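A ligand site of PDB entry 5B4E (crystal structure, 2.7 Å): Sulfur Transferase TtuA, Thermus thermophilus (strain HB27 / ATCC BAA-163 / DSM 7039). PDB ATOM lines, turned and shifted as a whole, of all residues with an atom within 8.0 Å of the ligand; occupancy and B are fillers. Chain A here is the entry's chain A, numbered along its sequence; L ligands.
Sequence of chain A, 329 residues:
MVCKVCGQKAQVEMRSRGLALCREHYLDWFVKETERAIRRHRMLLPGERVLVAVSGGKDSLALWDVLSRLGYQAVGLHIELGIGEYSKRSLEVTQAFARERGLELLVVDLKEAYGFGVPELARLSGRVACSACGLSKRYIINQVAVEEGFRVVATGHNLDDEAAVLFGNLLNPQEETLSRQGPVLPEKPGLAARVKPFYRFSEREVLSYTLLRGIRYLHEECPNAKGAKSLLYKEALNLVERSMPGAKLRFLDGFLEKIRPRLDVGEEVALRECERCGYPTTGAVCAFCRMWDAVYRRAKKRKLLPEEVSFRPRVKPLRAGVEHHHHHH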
ATOM      1  N   LEU A  81      -7.586 -12.798   7.478  1.00  0.00           N
ATOM      2  CA  LEU A  81      -7.362 -12.943   8.906  1.00  0.00           C
ATOM      3  C   LEU A  81      -7.329 -11.605   9.650  1.00  0.00           C
ATOM      4  O   LEU A  81      -7.209 -11.567  10.866  1.00  0.00           O
ATOM      5  CB  LEU A  81      -6.068 -13.720   9.157  1.00  0.00           C
ATOM      6  CG  LEU A  81      -6.113 -15.155   8.625  1.00  0.00           C
ATOM      7  CD1 LEU A  81      -4.740 -15.800   8.691  1.00  0.00           C
ATOM      8  CD2 LEU A  81      -7.143 -15.971   9.381  1.00  0.00           C
ATOM      9  N   ILE A  83      -5.123  -9.257   9.735  1.00  0.00           N
ATOM     10  CA  ILE A  83      -3.843  -8.866  10.313  1.00  0.00           C
ATOM     11  C   ILE A  83      -3.268  -7.658   9.576  1.00  0.00           C
ATOM     12  O   ILE A  83      -2.248  -7.752   8.892  1.00  0.00           O
ATOM     13  CB  ILE A  83      -2.819 -10.033  10.290  1.00  0.00           C
ATOM     14  CG1 ILE A  83      -3.491 -11.327  10.765  1.00  0.00           C
ATOM     15  CG2 ILE A  83      -1.614  -9.717  11.169  1.00  0.00           C
ATOM     16  CD1 ILE A  83      -2.530 -12.494  10.892  1.00  0.00           C
ATOM     17  N   TYR A  86      -1.104  -6.374   5.966  1.00  0.00           N
ATOM     18  CA  TYR A  86      -0.616  -7.687   5.558  1.00  0.00           C
ATOM     19  C   TYR A  86      -1.723  -8.529   4.938  1.00  0.00           C
ATOM     20  O   TYR A  86      -1.626  -8.905   3.755  1.00  0.00           O
ATOM     21  CB  TYR A  86      -0.010  -8.422   6.761  1.00  0.00           C
ATOM     22  CG  TYR A  86       0.294  -9.878   6.492  1.00  0.00           C
ATOM     23  CD1 TYR A  86       1.360 -10.241   5.670  1.00  0.00           C
ATOM     24  CD2 TYR A  86      -0.473 -10.893   7.061  1.00  0.00           C
ATOM     25  CE1 TYR A  86       1.645 -11.571   5.415  1.00  0.00           C
ATOM     26  CE2 TYR A  86      -0.186 -12.222   6.817  1.00  0.00           C
ATOM     27  CZ  TYR A  86       0.875 -12.554   5.993  1.00  0.00           C
ATOM     28  OH  TYR A  86       1.178 -13.875   5.735  1.00  0.00           O
ATOM     29  N   SER A  87      -2.753  -8.836   5.725  1.00  0.00           N
ATOM     30  CA  SER A  87      -3.907  -9.590   5.227  1.00  0.00           C
ATOM     31  C   SER A  87      -4.567  -8.929   4.017  1.00  0.00           C
ATOM     32  O   SER A  87      -5.137  -9.611   3.172  1.00  0.00           O
ATOM     33  CB  SER A  87      -4.934  -9.760   6.338  1.00  0.00           C
ATOM     34  OG  SER A  87      -4.511 -10.681   7.329  1.00  0.00           O
ATOM     35  N   VAL A 118      -7.657 -11.776  13.759  1.00  0.00           N
ATOM     36  CA  VAL A 118      -6.701 -12.539  14.557  1.00  0.00           C
ATOM     37  C   VAL A 118      -6.044 -11.721  15.693  1.00  0.00           C
ATOM     38  O   VAL A 118      -5.916 -12.233  16.808  1.00  0.00           O
ATOM     39  CB  VAL A 118      -5.593 -13.163  13.657  1.00  0.00           C
ATOM     40  CG1 VAL A 118      -4.406 -13.636  14.478  1.00  0.00           C
ATOM     41  CG2 VAL A 118      -6.174 -14.315  12.839  1.00  0.00           C
ATOM     42  N   PRO A 119      -5.637 -10.455  15.432  1.00  0.00           N
ATOM     43  CA  PRO A 119      -5.030  -9.686  16.529  1.00  0.00           C
ATOM     44  C   PRO A 119      -5.906  -9.551  17.776  1.00  0.00           C
ATOM     45  O   PRO A 119      -5.450  -9.889  18.870  1.00  0.00           O
ATOM     46  CB  PRO A 119      -4.787  -8.313  15.890  1.00  0.00           C
ATOM     47  CG  PRO A 119      -4.583  -8.610  14.462  1.00  0.00           C
ATOM     48  CD  PRO A 119      -5.535  -9.721  14.153  1.00  0.00           C
ATOM     49  N   VAL A 128      -2.219 -17.915  22.217  1.00  0.00           N
ATOM     50  CA  VAL A 128      -1.287 -17.219  21.334  1.00  0.00           C
ATOM     51  C   VAL A 128      -1.986 -16.985  20.001  1.00  0.00           C
ATOM     52  O   VAL A 128      -2.918 -17.712  19.660  1.00  0.00           O
ATOM     53  CB  VAL A 128       0.009 -18.016  21.119  1.00  0.00           C
ATOM     54  CG1 VAL A 128       1.160 -17.081  20.782  1.00  0.00           C
ATOM     55  CG2 VAL A 128       0.340 -18.850  22.350  1.00  0.00           C
ATOM     56  N   ALA A 129      -1.539 -15.968  19.267  1.00  0.00           N
ATOM     57  CA  ALA A 129      -2.171 -15.597  18.005  1.00  0.00           C
ATOM     58  C   ALA A 129      -2.273 -16.791  17.058  1.00  0.00           C
ATOM     59  O   ALA A 129      -3.304 -17.039  16.441  1.00  0.00           O
ATOM     60  CB  ALA A 129      -1.402 -14.468  17.346  1.00  0.00           C
ATOM     61  N   CYS A 130      -1.172 -17.521  16.968  1.00  0.00           N
ATOM     62  CA  CYS A 130      -1.088 -18.673  16.091  1.00  0.00           C
ATOM     63  C   CYS A 130      -2.088 -19.777  16.449  1.00  0.00           C
ATOM     64  O   CYS A 130      -2.577 -20.463  15.541  1.00  0.00           O
ATOM     65  CB  CYS A 130       0.345 -19.196  16.088  1.00  0.00           C
ATOM     66  SG  CYS A 130       1.489 -18.027  15.339  1.00  0.00           S
ATOM     67  N   SER A 131      -2.382 -19.946  17.743  1.00  0.00           N
ATOM     68  CA  SER A 131      -3.325 -20.975  18.188  1.00  0.00           C
ATOM     69  C   SER A 131      -4.763 -20.692  17.744  1.00  0.00           C
ATOM     70  O   SER A 131      -5.448 -21.571  17.195  1.00  0.00           O
ATOM     71  CB  SER A 131      -3.259 -21.114  19.710  1.00  0.00           C
ATOM     72  OG  SER A 131      -3.947 -22.257  20.155  1.00  0.00           O
ATOM     73  N   ALA A 132      -5.227 -19.490  18.035  1.00  0.00           N
ATOM     74  CA  ALA A 132      -6.563 -19.051  17.655  1.00  0.00           C
ATOM     75  C   ALA A 132      -6.694 -18.982  16.138  1.00  0.00           C
ATOM     76  O   ALA A 132      -7.737 -19.337  15.582  1.00  0.00           O
ATOM     77  CB  ALA A 132      -6.872 -17.712  18.288  1.00  0.00           C
ATOM     78  N   CYS A 133      -5.630 -18.544  15.477  1.00  0.00           N
ATOM     79  CA  CYS A 133      -5.632 -18.372  14.024  1.00  0.00           C
ATOM     80  C   CYS A 133      -5.721 -19.706  13.299  1.00  0.00           C
ATOM     81  O   CYS A 133      -6.530 -19.871  12.389  1.00  0.00           O
ATOM     82  CB  CYS A 133      -4.388 -17.614  13.565  1.00  0.00           C
ATOM     83  SG  CYS A 133      -4.274 -17.392  11.776  1.00  0.00           S
ATOM     84  N   GLY A 134      -4.863 -20.645  13.698  1.00  0.00           N
ATOM     85  CA  GLY A 134      -4.849 -21.959  13.087  1.00  0.00           C
ATOM     86  C   GLY A 134      -6.176 -22.647  13.300  1.00  0.00           C
ATOM     87  O   GLY A 134      -6.731 -23.254  12.386  1.00  0.00           O
ATOM     88  N   LEU A 135      -6.698 -22.540  14.526  1.00  0.00           N
ATOM     89  CA  LEU A 135      -7.979 -23.137  14.877  1.00  0.00           C
ATOM     90  C   LEU A 135      -9.094 -22.603  13.990  1.00  0.00           C
ATOM     91  O   LEU A 135      -9.934 -23.361  13.505  1.00  0.00           O
ATOM     92  CB  LEU A 135      -8.294 -22.876  16.344  1.00  0.00           C
ATOM     93  CG  LEU A 135      -9.592 -23.482  16.881  1.00  0.00           C
ATOM     94  CD1 LEU A 135      -9.637 -24.963  16.576  1.00  0.00           C
ATOM     95  CD2 LEU A 135      -9.716 -23.245  18.382  1.00  0.00           C
ATOM     96  N   LYS A 137      -8.681 -21.170  10.987  1.00  0.00           N
ATOM     97  CA  LYS A 137      -8.406 -21.542   9.605  1.00  0.00           C
ATOM     98  C   LYS A 137      -8.894 -22.951   9.280  1.00  0.00           C
ATOM     99  O   LYS A 137      -9.601 -23.163   8.298  1.00  0.00           O
ATOM    100  CB  LYS A 137      -6.903 -21.416   9.298  1.00  0.00           C
ATOM    101  CG  LYS A 137      -6.419 -19.975   9.145  1.00  0.00           C
ATOM    102  CD  LYS A 137      -4.936 -19.904   8.764  1.00  0.00           C
ATOM    103  CE  LYS A 137      -4.050 -20.548   9.826  1.00  0.00           C
ATOM    104  NZ  LYS A 137      -2.598 -20.415   9.506  1.00  0.00           N
ATOM    105  N   ARG A 138      -8.543 -23.921  10.124  1.00  0.00           N
ATOM    106  CA  ARG A 138      -8.911 -25.312   9.881  1.00  0.00           C
ATOM    107  C   ARG A 138     -10.424 -25.544   9.964  1.00  0.00           C
ATOM    108  O   ARG A 138     -10.986 -26.290   9.163  1.00  0.00           O
ATOM    109  CB  ARG A 138      -8.189 -26.234  10.878  1.00  0.00           C
ATOM    110  CG  ARG A 138      -6.697 -25.957  10.926  1.00  0.00           C
ATOM    111  CD  ARG A 138      -5.886 -27.057  11.598  1.00  0.00           C
ATOM    112  NE  ARG A 138      -4.555 -26.571  11.979  1.00  0.00           N
ATOM    113  CZ  ARG A 138      -3.574 -26.313  11.112  1.00  0.00           C
ATOM    114  NH1 ARG A 138      -3.750 -26.493   9.813  1.00  0.00           N
ATOM    115  NH2 ARG A 138      -2.408 -25.881  11.562  1.00  0.00           N
ATOM    116  N   GLU A 221       6.004 -12.258   4.913  1.00  0.00           N
ATOM    117  CA  GLU A 221       5.330 -13.203   5.798  1.00  0.00           C
ATOM    118  C   GLU A 221       4.692 -12.479   6.974  1.00  0.00           C
ATOM    119  O   GLU A 221       5.164 -11.406   7.368  1.00  0.00           O
ATOM    120  CB  GLU A 221       6.324 -14.251   6.307  1.00  0.00           C
ATOM    121  CG  GLU A 221       5.706 -15.392   7.127  1.00  0.00           C
ATOM    122  CD  GLU A 221       4.516 -16.040   6.433  1.00  0.00           C
ATOM    123  OE1 GLU A 221       3.503 -16.281   7.122  1.00  0.00           O
ATOM    124  OE2 GLU A 221       4.590 -16.338   5.218  1.00  0.00           O
ATOM    125  N   CYS A 222       3.620 -13.056   7.515  1.00  0.00           N
ATOM    126  CA  CYS A 222       2.999 -12.561   8.746  1.00  0.00           C
ATOM    127  C   CYS A 222       4.004 -12.146   9.811  1.00  0.00           C
ATOM    128  O   CYS A 222       5.062 -12.765   9.922  1.00  0.00           O
ATOM    129  CB  CYS A 222       2.106 -13.631   9.339  1.00  0.00           C
ATOM    130  SG  CYS A 222       1.088 -13.142  10.763  1.00  0.00           S
ATOM    131  N   PRO A 223       3.706 -11.085  10.575  1.00  0.00           N
ATOM    132  CA  PRO A 223       4.398 -11.017  11.865  1.00  0.00           C
ATOM    133  C   PRO A 223       4.040 -12.213  12.752  1.00  0.00           C
ATOM    134  O   PRO A 223       3.345 -12.027  13.765  1.00  0.00           O
ATOM    135  CB  PRO A 223       3.896  -9.689  12.477  1.00  0.00           C
ATOM    136  CG  PRO A 223       3.218  -8.959  11.367  1.00  0.00           C
ATOM    137  CD  PRO A 223       2.794  -9.937  10.350  1.00  0.00           C
ATOM    138  N   ASN A 224       4.501 -13.405  12.358  1.00  0.00           N
ATOM    139  CA  ASN A 224       4.193 -14.653  13.059  1.00  0.00           C
ATOM    140  C   ASN A 224       4.585 -14.620  14.539  1.00  0.00           C
ATOM    141  O   ASN A 224       5.379 -13.762  14.941  1.00  0.00           O
ATOM    142  CB  ASN A 224       4.866 -15.857  12.361  1.00  0.00           C
ATOM    143  CG  ASN A 224       6.340 -15.623  12.019  1.00  0.00           C
ATOM    144  OD1 ASN A 224       6.712 -15.560  10.843  1.00  0.00           O
ATOM    145  ND2 ASN A 224       7.172 -15.480  13.049  1.00  0.00           N
ATOM    146  N   ALA A 225       4.027 -15.537  15.332  1.00  0.00           N
ATOM    147  CA  ALA A 225       4.345 -15.599  16.760  1.00  0.00           C
ATOM    148  C   ALA A 225       5.015 -16.942  17.047  1.00  0.00           C
ATOM    149  O   ALA A 225       6.197 -17.010  17.401  1.00  0.00           O
ATOM    150  CB  ALA A 225       3.089 -15.426  17.625  1.00  0.00           C
ATOM    151  N   LYS A 226       4.234 -18.009  16.912  1.00  0.00           N
ATOM    152  CA  LYS A 226       4.758 -19.338  17.128  1.00  0.00           C
ATOM    153  C   LYS A 226       4.925 -20.106  15.824  1.00  0.00           C
ATOM    154  O   LYS A 226       5.064 -21.344  15.837  1.00  0.00           O
ATOM    155  CB  LYS A 226       3.868 -20.102  18.102  1.00  0.00           C
ATOM    156  CG  LYS A 226       4.055 -19.634  19.529  1.00  0.00           C
ATOM    157  CD  LYS A 226       3.886 -20.787  20.505  1.00  0.00           C
ATOM    158  CE  LYS A 226       4.363 -20.404  21.895  1.00  0.00           C
ATOM    159  NZ  LYS A 226       4.223 -21.531  22.855  1.00  0.00           N
ATOM    160  N   GLY A 227       4.915 -19.385  14.705  1.00  0.00           N
ATOM    161  CA  GLY A 227       5.364 -19.937  13.432  1.00  0.00           C
ATOM    162  C   GLY A 227       6.866 -19.723  13.362  1.00  0.00           C
ATOM    163  O   GLY A 227       7.539 -20.123  12.419  1.00  0.00           O
ATOM    164  N   ALA A 228       7.375 -19.072  14.401  1.00  0.00           N
ATOM    165  CA  ALA A 228       8.809 -18.894  14.597  1.00  0.00           C
ATOM    166  C   ALA A 228       9.415 -20.226  14.994  1.00  0.00           C
ATOM    167  O   ALA A 228      10.610 -20.455  14.852  1.00  0.00           O
ATOM    168  CB  ALA A 228       9.071 -17.854  15.654  1.00  0.00           C
HETATM  169 FE1  LIG L   1       0.190 -15.187  11.218  1.00  0.00          FE
HETATM  170 FE2  LIG L   1       0.750 -17.338  13.257  1.00  0.00          FE
HETATM  171 FE3  LIG L   1       0.312 -18.059  10.417  1.00  0.00          FE
HETATM  172 FE4  LIG L   1      -2.001 -17.077  11.998  1.00  0.00          FE
HETATM  173  S1  LIG L   1      -0.589 -18.662  12.253  1.00  0.00           S
HETATM  174  S2  LIG L   1      -1.120 -16.485  10.146  1.00  0.00           S
HETATM  175  S3  LIG L   1      -0.687 -15.766  13.068  1.00  0.00           S
HETATM  176  S4  LIG L   1       1.646 -16.726  11.412  1.00  0.00           S
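The side-chain sulfur (SG) of Cys 222 binds an iron atom (FE1) of the ligand (2.3 Å). The side-chain sulfur (SG) of Cys 133 binds an iron atom (FE4) of the ligand (2.3 Å). FE2 of the ligand is bound by SG of Cys 130, 2.3 Å away.
The backbone carbonyl oxygen (O) of Cys 222 sits close to the side-chain amide oxygen (OD1) of Asn 224 (3.4 Å). N of Cys 222 is in hydrogen-bond range of OH of Tyr 86. N of Ala 225 sits close to SG of Cys 130 (3.6 Å). N of Gly 227 sits close to SG of Cys 130 (3.7 Å). SG of Cys 130 sits close to N of Lys 226. OG of Ser 87 lies within hydrogen-bond range of N of Ile 83. O of Leu 81 is in hydrogen-bond range of N of Val 118 (2.9 Å).
Leu 81 touches the ligand. Ile 83 touches the ligand. Lys 137 touches the ligand (NZ to S1, 3.8 Å). Asn 224 touches the ligand (CB to S4, 3.5 Å). Hydrophobic or aromatic side chains within 4 Å of the ligand: Leu 81 and Ile 83. Within 4 Å of the ligand: Leu 81, Ile 83, Cys 130, Cys 133, Lys 137, Cys 222 and Asn 224. The nearest printed residue that does not touch the ligand is Ala 225 (4.3 Å).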
